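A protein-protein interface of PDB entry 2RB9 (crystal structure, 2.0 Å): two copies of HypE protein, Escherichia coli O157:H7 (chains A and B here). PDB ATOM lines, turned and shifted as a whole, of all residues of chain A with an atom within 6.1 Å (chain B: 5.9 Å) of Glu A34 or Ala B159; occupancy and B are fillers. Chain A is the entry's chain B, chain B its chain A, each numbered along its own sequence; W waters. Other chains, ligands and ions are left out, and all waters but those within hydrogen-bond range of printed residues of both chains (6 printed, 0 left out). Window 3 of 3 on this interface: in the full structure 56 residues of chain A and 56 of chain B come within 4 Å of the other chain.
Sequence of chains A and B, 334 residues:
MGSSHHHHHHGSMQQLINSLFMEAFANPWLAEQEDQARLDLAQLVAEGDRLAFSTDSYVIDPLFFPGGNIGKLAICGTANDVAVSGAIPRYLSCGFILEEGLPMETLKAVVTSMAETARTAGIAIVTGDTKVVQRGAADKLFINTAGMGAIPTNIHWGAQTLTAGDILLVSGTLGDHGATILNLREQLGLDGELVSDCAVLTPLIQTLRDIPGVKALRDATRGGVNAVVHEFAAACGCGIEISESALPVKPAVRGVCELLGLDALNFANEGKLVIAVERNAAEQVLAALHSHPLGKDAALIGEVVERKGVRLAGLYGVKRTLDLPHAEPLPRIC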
ATOM      1  N   GLU A  32     -26.772 -15.029   1.154  1.00  0.00           N
ATOM      2  CA  GLU A  32     -26.521 -15.280   2.584  1.00  0.00           C
ATOM      3  C   GLU A  32     -26.099 -16.737   2.868  1.00  0.00           C
ATOM      4  O   GLU A  32     -26.257 -17.251   3.980  1.00  0.00           O
ATOM      5  CB  GLU A  32     -27.716 -14.829   3.452  1.00  0.00           C
ATOM      6  CG  GLU A  32     -27.453 -14.816   4.969  1.00  0.00           C
ATOM      7  CD  GLU A  32     -26.048 -14.332   5.341  1.00  0.00           C
ATOM      8  OE1 GLU A  32     -25.770 -13.115   5.198  1.00  0.00           O
ATOM      9  OE2 GLU A  32     -25.227 -15.176   5.780  1.00  0.00           O
ATOM     10  N   GLN A  33     -25.549 -17.384   1.847  1.00  0.00           N
ATOM     11  CA  GLN A  33     -25.072 -18.749   1.966  1.00  0.00           C
ATOM     12  C   GLN A  33     -23.741 -18.787   2.706  1.00  0.00           C
ATOM     13  O   GLN A  33     -22.911 -17.899   2.542  1.00  0.00           O
ATOM     14  CB  GLN A  33     -24.912 -19.366   0.573  1.00  0.00           C
ATOM     15  CG  GLN A  33     -24.386 -20.784   0.570  1.00  0.00           C
ATOM     16  CD  GLN A  33     -24.371 -21.388  -0.814  1.00  0.00           C
ATOM     17  OE1 GLN A  33     -25.348 -21.283  -1.556  1.00  0.00           O
ATOM     18  NE2 GLN A  33     -23.266 -22.026  -1.167  1.00  0.00           N
ATOM     19  N   GLU A  34     -23.555 -19.819   3.524  1.00  0.00           N
ATOM     20  CA  GLU A  34     -22.260 -20.083   4.137  1.00  0.00           C
ATOM     21  C   GLU A  34     -21.476 -21.136   3.333  1.00  0.00           C
ATOM     22  O   GLU A  34     -21.135 -20.873   2.184  1.00  0.00           O
ATOM     23  CB  GLU A  34     -22.415 -20.424   5.618  1.00  0.00           C
ATOM     24  CG  GLU A  34     -22.764 -19.191   6.462  1.00  0.00           C
ATOM     25  CD  GLU A  34     -23.152 -19.538   7.888  1.00  0.00           C
ATOM     26  OE1 GLU A  34     -24.151 -20.263   8.079  1.00  0.00           O
ATOM     27  OE2 GLU A  34     -22.459 -19.075   8.819  1.00  0.00           O
ATOM     28  N   ASP A  35     -21.198 -22.308   3.909  1.00  0.00           N
ATOM     29  CA  ASP A  35     -20.355 -23.316   3.228  1.00  0.00           C
ATOM     30  C   ASP A  35     -21.111 -24.298   2.318  1.00  0.00           C
ATOM     31  O   ASP A  35     -20.493 -25.146   1.661  1.00  0.00           O
ATOM     32  CB  ASP A  35     -19.522 -24.096   4.244  1.00  0.00           C
ATOM     33  CG  ASP A  35     -18.479 -23.231   4.928  1.00  0.00           C
ATOM     34  OD1 ASP A  35     -17.801 -22.432   4.234  1.00  0.00           O
ATOM     35  OD2 ASP A  35     -18.333 -23.363   6.162  1.00  0.00           O
ATOM     36  N   GLN A  36     -22.438 -24.178   2.290  1.00  0.00           N
ATOM     37  CA  GLN A  36     -23.300 -25.110   1.558  1.00  0.00           C
ATOM     38  C   GLN A  36     -24.659 -24.484   1.275  1.00  0.00           C
ATOM     39  O   GLN A  36     -25.112 -23.614   2.027  1.00  0.00           O
ATOM     40  CB  GLN A  36     -23.455 -26.435   2.338  1.00  0.00           C
ATOM     41  CG  GLN A  36     -24.398 -26.430   3.558  1.00  0.00           C
ATOM     42  CD  GLN A  36     -23.935 -25.522   4.699  1.00  0.00           C
ATOM     43  OE1 GLN A  36     -24.665 -24.615   5.113  1.00  0.00           O
ATOM     44  NE2 GLN A  36     -22.727 -25.766   5.214  1.00  0.00           N
ATOM     45  N   ARG A  38     -28.772 -25.025   1.162  1.00  0.00           N
ATOM     46  CA  ARG A  38     -29.698 -25.771   2.009  1.00  0.00           C
ATOM     47  C   ARG A  38     -31.054 -25.863   1.317  1.00  0.00           C
ATOM     48  O   ARG A  38     -31.740 -24.861   1.138  1.00  0.00           O
ATOM     49  CB  ARG A  38     -29.809 -25.107   3.388  1.00  0.00           C
ATOM     50  CG  ARG A  38     -28.459 -25.012   4.099  1.00  0.00           C
ATOM     51  CD  ARG A  38     -28.587 -24.533   5.524  1.00  0.00           C
ATOM     52  NE  ARG A  38     -27.267 -24.437   6.146  1.00  0.00           N
ATOM     53  CZ  ARG A  38     -27.052 -24.065   7.405  1.00  0.00           C
ATOM     54  NH1 ARG A  38     -28.075 -23.754   8.193  1.00  0.00           N
ATOM     55  NH2 ARG A  38     -25.811 -24.003   7.876  1.00  0.00           N
ATOM     56  N   TRP B 157     -27.653 -23.882  12.760  1.00  0.00           N
ATOM     57  CA  TRP B 157     -26.386 -23.169  12.827  1.00  0.00           C
ATOM     58  C   TRP B 157     -26.247 -22.206  11.652  1.00  0.00           C
ATOM     59  O   TRP B 157     -26.388 -22.600  10.486  1.00  0.00           O
ATOM     60  CB  TRP B 157     -25.205 -24.148  12.862  1.00  0.00           C
ATOM     61  CG  TRP B 157     -25.183 -25.093  14.052  1.00  0.00           C
ATOM     62  CD1 TRP B 157     -25.760 -24.898  15.281  1.00  0.00           C
ATOM     63  CD2 TRP B 157     -24.504 -26.356  14.128  1.00  0.00           C
ATOM     64  NE1 TRP B 157     -25.499 -25.971  16.103  1.00  0.00           N
ATOM     65  CE2 TRP B 157     -24.736 -26.881  15.417  1.00  0.00           C
ATOM     66  CE3 TRP B 157     -23.737 -27.102  13.220  1.00  0.00           C
ATOM     67  CZ2 TRP B 157     -24.220 -28.119  15.829  1.00  0.00           C
ATOM     68  CZ3 TRP B 157     -23.226 -28.333  13.628  1.00  0.00           C
ATOM     69  CH2 TRP B 157     -23.468 -28.827  14.923  1.00  0.00           C
ATOM     70  N   GLY B 158     -25.966 -20.946  11.973  1.00  0.00           N
ATOM     71  CA  GLY B 158     -25.776 -19.894  10.978  1.00  0.00           C
ATOM     72  C   GLY B 158     -25.269 -18.625  11.634  1.00  0.00           C
ATOM     73  O   GLY B 158     -25.600 -18.346  12.783  1.00  0.00           O
ATOM     74  N   ALA B 159     -24.471 -17.856  10.898  1.00  0.00           N
ATOM     75  CA  ALA B 159     -23.834 -16.649  11.433  1.00  0.00           C
ATOM     76  C   ALA B 159     -24.793 -15.469  11.592  1.00  0.00           C
ATOM     77  O   ALA B 159     -24.513 -14.547  12.366  1.00  0.00           O
ATOM     78  CB  ALA B 159     -22.639 -16.259  10.580  1.00  0.00           C
ATOM     79  N   GLN B 160     -25.918 -15.508  10.871  1.00  0.00           N
ATOM     80  CA  GLN B 160     -26.955 -14.478  10.977  1.00  0.00           C
ATOM     81  C   GLN B 160     -27.491 -14.363  12.397  1.00  0.00           C
ATOM     82  O   GLN B 160     -28.019 -13.324  12.784  1.00  0.00           O
ATOM     83  CB  GLN B 160     -28.121 -14.766  10.022  1.00  0.00           C
ATOM     84  CG  GLN B 160     -28.015 -14.093   8.659  1.00  0.00           C
ATOM     85  CD  GLN B 160     -29.295 -14.213   7.836  1.00  0.00           C
ATOM     86  OE1 GLN B 160     -29.876 -15.296   7.713  1.00  0.00           O
ATOM     87  NE2 GLN B 160     -29.731 -13.098   7.259  1.00  0.00           N
ATOM     88  N   THR B 161     -27.348 -15.439  13.169  1.00  0.00           N
ATOM     89  CA  THR B 161     -27.895 -15.517  14.522  1.00  0.00           C
ATOM     90  C   THR B 161     -27.010 -14.891  15.597  1.00  0.00           C
ATOM     91  O   THR B 161     -27.455 -14.715  16.732  1.00  0.00           O
ATOM     92  CB  THR B 161     -28.203 -16.978  14.932  1.00  0.00           C
ATOM     93  OG1 THR B 161     -26.983 -17.725  15.023  1.00  0.00           O
ATOM     94  CG2 THR B 161     -29.141 -17.646  13.927  1.00  0.00           C
ATOM     95  N   LEU B 162     -25.768 -14.557  15.250  1.00  0.00           N
ATOM     96  CA  LEU B 162     -24.810 -14.059  16.244  1.00  0.00           C
ATOM     97  C   LEU B 162     -25.180 -12.685  16.797  1.00  0.00           C
ATOM     98  O   LEU B 162     -25.683 -11.825  16.073  1.00  0.00           O
ATOM     99  CB  LEU B 162     -23.379 -14.056  15.694  1.00  0.00           C
ATOM    100  CG  LEU B 162     -22.846 -15.382  15.129  1.00  0.00           C
ATOM    101  CD1 LEU B 162     -21.379 -15.246  14.714  1.00  0.00           C
ATOM    102  CD2 LEU B 162     -23.033 -16.526  16.127  1.00  0.00           C
ATOM    103  N   LYS B 215     -24.018 -21.796  17.949  1.00  0.00           N
ATOM    104  CA  LYS B 215     -24.777 -20.886  17.084  1.00  0.00           C
ATOM    105  C   LYS B 215     -24.332 -20.825  15.619  1.00  0.00           C
ATOM    106  O   LYS B 215     -25.160 -20.612  14.727  1.00  0.00           O
ATOM    107  CB  LYS B 215     -24.811 -19.480  17.685  1.00  0.00           C
ATOM    108  CG  LYS B 215     -25.640 -19.384  18.968  1.00  0.00           C
ATOM    109  CD  LYS B 215     -25.608 -17.980  19.563  1.00  0.00           C
ATOM    110  CE  LYS B 215     -26.581 -17.039  18.862  1.00  0.00           C
ATOM    111  NZ  LYS B 215     -26.479 -15.636  19.379  1.00  0.00           N
ATOM    112  N   ALA B 216     -23.031 -20.993  15.377  1.00  0.00           N
ATOM    113  CA  ALA B 216     -22.478 -20.959  14.023  1.00  0.00           C
ATOM    114  C   ALA B 216     -21.210 -21.793  13.946  1.00  0.00           C
ATOM    115  O   ALA B 216     -20.449 -21.879  14.917  1.00  0.00           O
ATOM    116  CB  ALA B 216     -22.201 -19.528  13.582  1.00  0.00           C
ATOM    117  N   LEU B 217     -21.001 -22.403  12.782  1.00  0.00           N
ATOM    118  CA  LEU B 217     -19.871 -23.287  12.527  1.00  0.00           C
ATOM    119  C   LEU B 217     -19.471 -23.165  11.083  1.00  0.00           C
ATOM    120  O   LEU B 217     -20.322 -23.255  10.197  1.00  0.00           O
ATOM    121  CB  LEU B 217     -20.258 -24.746  12.758  1.00  0.00           C
ATOM    122  CG  LEU B 217     -19.591 -25.598  13.821  1.00  0.00           C
ATOM    123  CD1 LEU B 217     -20.398 -25.477  15.084  1.00  0.00           C
ATOM    124  CD2 LEU B 217     -19.588 -27.040  13.360  1.00  0.00           C
ATOM    125  N   ARG B 218     -18.179 -22.970  10.847  1.00  0.00           N
ATOM    126  CA  ARG B 218     -17.637 -22.953   9.496  1.00  0.00           C
ATOM    127  C   ARG B 218     -16.242 -23.545   9.506  1.00  0.00           C
ATOM    128  O   ARG B 218     -15.508 -23.402  10.487  1.00  0.00           O
ATOM    129  CB  ARG B 218     -17.604 -21.528   8.925  1.00  0.00           C
ATOM    130  CG  ARG B 218     -18.977 -20.991   8.554  1.00  0.00           C
ATOM    131  CD  ARG B 218     -18.909 -19.769   7.687  1.00  0.00           C
ATOM    132  NE  ARG B 218     -18.550 -20.091   6.312  1.00  0.00           N
ATOM    133  CZ  ARG B 218     -18.722 -19.264   5.285  1.00  0.00           C
ATOM    134  NH1 ARG B 218     -19.260 -18.063   5.477  1.00  0.00           N
ATOM    135  NH2 ARG B 218     -18.364 -19.638   4.062  1.00  0.00           N
ATOM    136  N   GLU B 231     -16.696 -12.926   7.407  1.00  0.00           N
ATOM    137  CA  GLU B 231     -17.989 -13.478   6.995  1.00  0.00           C
ATOM    138  C   GLU B 231     -18.994 -13.486   8.149  1.00  0.00           C
ATOM    139  O   GLU B 231     -20.156 -13.131   7.953  1.00  0.00           O
ATOM    140  CB  GLU B 231     -17.824 -14.894   6.422  1.00  0.00           C
ATOM    141  CG  GLU B 231     -17.294 -14.921   4.994  1.00  0.00           C
ATOM    142  CD  GLU B 231     -16.414 -16.131   4.692  1.00  0.00           C
ATOM    143  OE1 GLU B 231     -16.324 -17.061   5.522  1.00  0.00           O
ATOM    144  OE2 GLU B 231     -15.800 -16.148   3.608  1.00  0.00           O
ATOM    145  N   PHE B 232     -18.548 -13.878   9.344  1.00  0.00           N
ATOM    146  CA  PHE B 232     -19.403 -13.875  10.545  1.00  0.00           C
ATOM    147  C   PHE B 232     -19.907 -12.468  10.881  1.00  0.00           C
ATOM    148  O   PHE B 232     -21.094 -12.275  11.182  1.00  0.00           O
ATOM    149  CB  PHE B 232     -18.644 -14.431  11.758  1.00  0.00           C
ATOM    150  CG  PHE B 232     -18.658 -15.938  11.883  1.00  0.00           C
ATOM    151  CD1 PHE B 232     -19.186 -16.754  10.880  1.00  0.00           C
ATOM    152  CD2 PHE B 232     -18.098 -16.542  13.009  1.00  0.00           C
ATOM    153  CE1 PHE B 232     -19.177 -18.140  11.012  1.00  0.00           C
ATOM    154  CE2 PHE B 232     -18.083 -17.933  13.149  1.00  0.00           C
ATOM    155  CZ  PHE B 232     -18.624 -18.733  12.147  1.00  0.00           C
ATOM    156  N   ALA B 235     -22.450 -11.077   8.373  1.00  0.00           N
ATOM    157  CA  ALA B 235     -23.726 -11.791   8.446  1.00  0.00           C
ATOM    158  C   ALA B 235     -24.627 -11.354   9.611  1.00  0.00           C
ATOM    159  O   ALA B 235     -25.853 -11.355   9.485  1.00  0.00           O
ATOM    160  CB  ALA B 235     -23.483 -13.293   8.495  1.00  0.00           C
ATOM    161  N   CYS B 236     -24.026 -10.993  10.740  1.00  0.00           N
ATOM    162  CA  CYS B 236     -24.795 -10.697  11.946  1.00  0.00           C
ATOM    163  C   CYS B 236     -24.899  -9.203  12.253  1.00  0.00           C
ATOM    164  O   CYS B 236     -25.608  -8.808  13.181  1.00  0.00           O
ATOM    165  CB  CYS B 236     -24.203 -11.432  13.150  1.00  0.00           C
ATOM    166  SG  CYS B 236     -22.602 -10.793  13.703  1.00  0.00           S
HETATM  167  O   HOH W   1     -20.406 -16.432   3.701  1.00  0.00           O
HETATM  168  O   HOH W   2     -22.807 -21.499  10.466  1.00  0.00           O
HETATM  169  O   HOH W   3     -27.953 -26.018  10.552  1.00  0.00           O
HETATM  170  O   HOH W   4     -23.131 -23.968   9.504  1.00  0.00           O
HETATM  171  O   HOH W   5     -20.741 -16.577   7.721  1.00  0.00           O
HETATM  172  O   HOH W   6     -15.628 -21.329   5.303  1.00  0.00           O
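The backbone NH (N) of Ala B159 lies within hydrogen-bond range of the side-chain carboxylate (OE2) of Glu A34 (3.1 Å). The guanidinium group (NH2) of Arg B218 lies within salt-bridge range of the side-chain carboxylate (OD1) of Asp A35 (2.9 Å). The backbone carbonyl oxygen (O) of Trp B157 sits at hydrogen-bond distance from the guanidinium group (NH2) of Arg A38, at 3.0 Å.
OG1 of Thr B161 lies within hydrogen-bond range of O of Gly B158, at 2.7 Å. The backbone carbonyl oxygen (O) of Lys B215 sits at hydrogen-bond distance from the backbone NH (N) of Gly B158 (2.9 Å). OE1 of Gln A36 sits at hydrogen-bond distance from NE of Arg A38, 2.8 Å away. The guanidinium group (NH1) of Arg B218 is in salt-bridge range of the side-chain carboxylate (OE1) of Glu B231, 3.1 Å away.
Glu A32 touches Gln B160. Ala B235 touches Glu A32 (CB to OE2, 3.7 Å). Glu A34 touches Gly B158 (OE1 to CA, 3.3 Å). Glu A34 touches Arg B218.
Of the printed residues of chain B, Glu A32 touches Gln B160 and Ala B235. Of the printed residues of chain B, Glu A34 touches Gly B158 (3.3 Å), Ala B159 (3.1 Å) and Arg B218 (3.5 Å). Printed residues of chain B within 4 Å of Asp A35: Arg B218. Of the printed residues of chain A, Trp B157 touches Arg A38. Ala B159 touches just one residue of chain A: Glu A34. Printed residues of chain A within 4 Å of Gln B160: Glu A32 (3.5 Å). Of the printed residues of chain A, Arg B218 touches Glu A34 (3.5 Å) and Asp A35 (2.9 Å).
Hydrophobic or aromatic side chains of chain B within 4 Å of the printed part of chain A: Ala B159 and Ala B235.
No position is printed for both chains. Of the 7 pairs that touch across the chains among the printed residues, none has its exchanged pair printed and touching as well.
Water W6 lies within hydrogen-bond range of the side-chain carboxylate of Asp A35 and the guanidinium group of Arg B218. Water W1 bridges NH1 of Arg B218 (2.7 Å) and O of Gln A33 (3.1 Å). Water W2 bridges OE2 of Glu A34 (3.0 Å) and O of Leu B217 (3.1 Å). Water W4 bridges the backbone carbonyl oxygen of Leu B217 (3.0 Å) and the guanidinium group of Arg A38 (3.1 Å). Water W5 bridges the guanidinium group (NH1) of Arg B218 and the side-chain carboxylate (OE2) of Glu A34. Water W3 lies within hydrogen-bond range of N of Trp B157 (3.1 Å) and NH1 of Arg A38 (3.3 Å).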
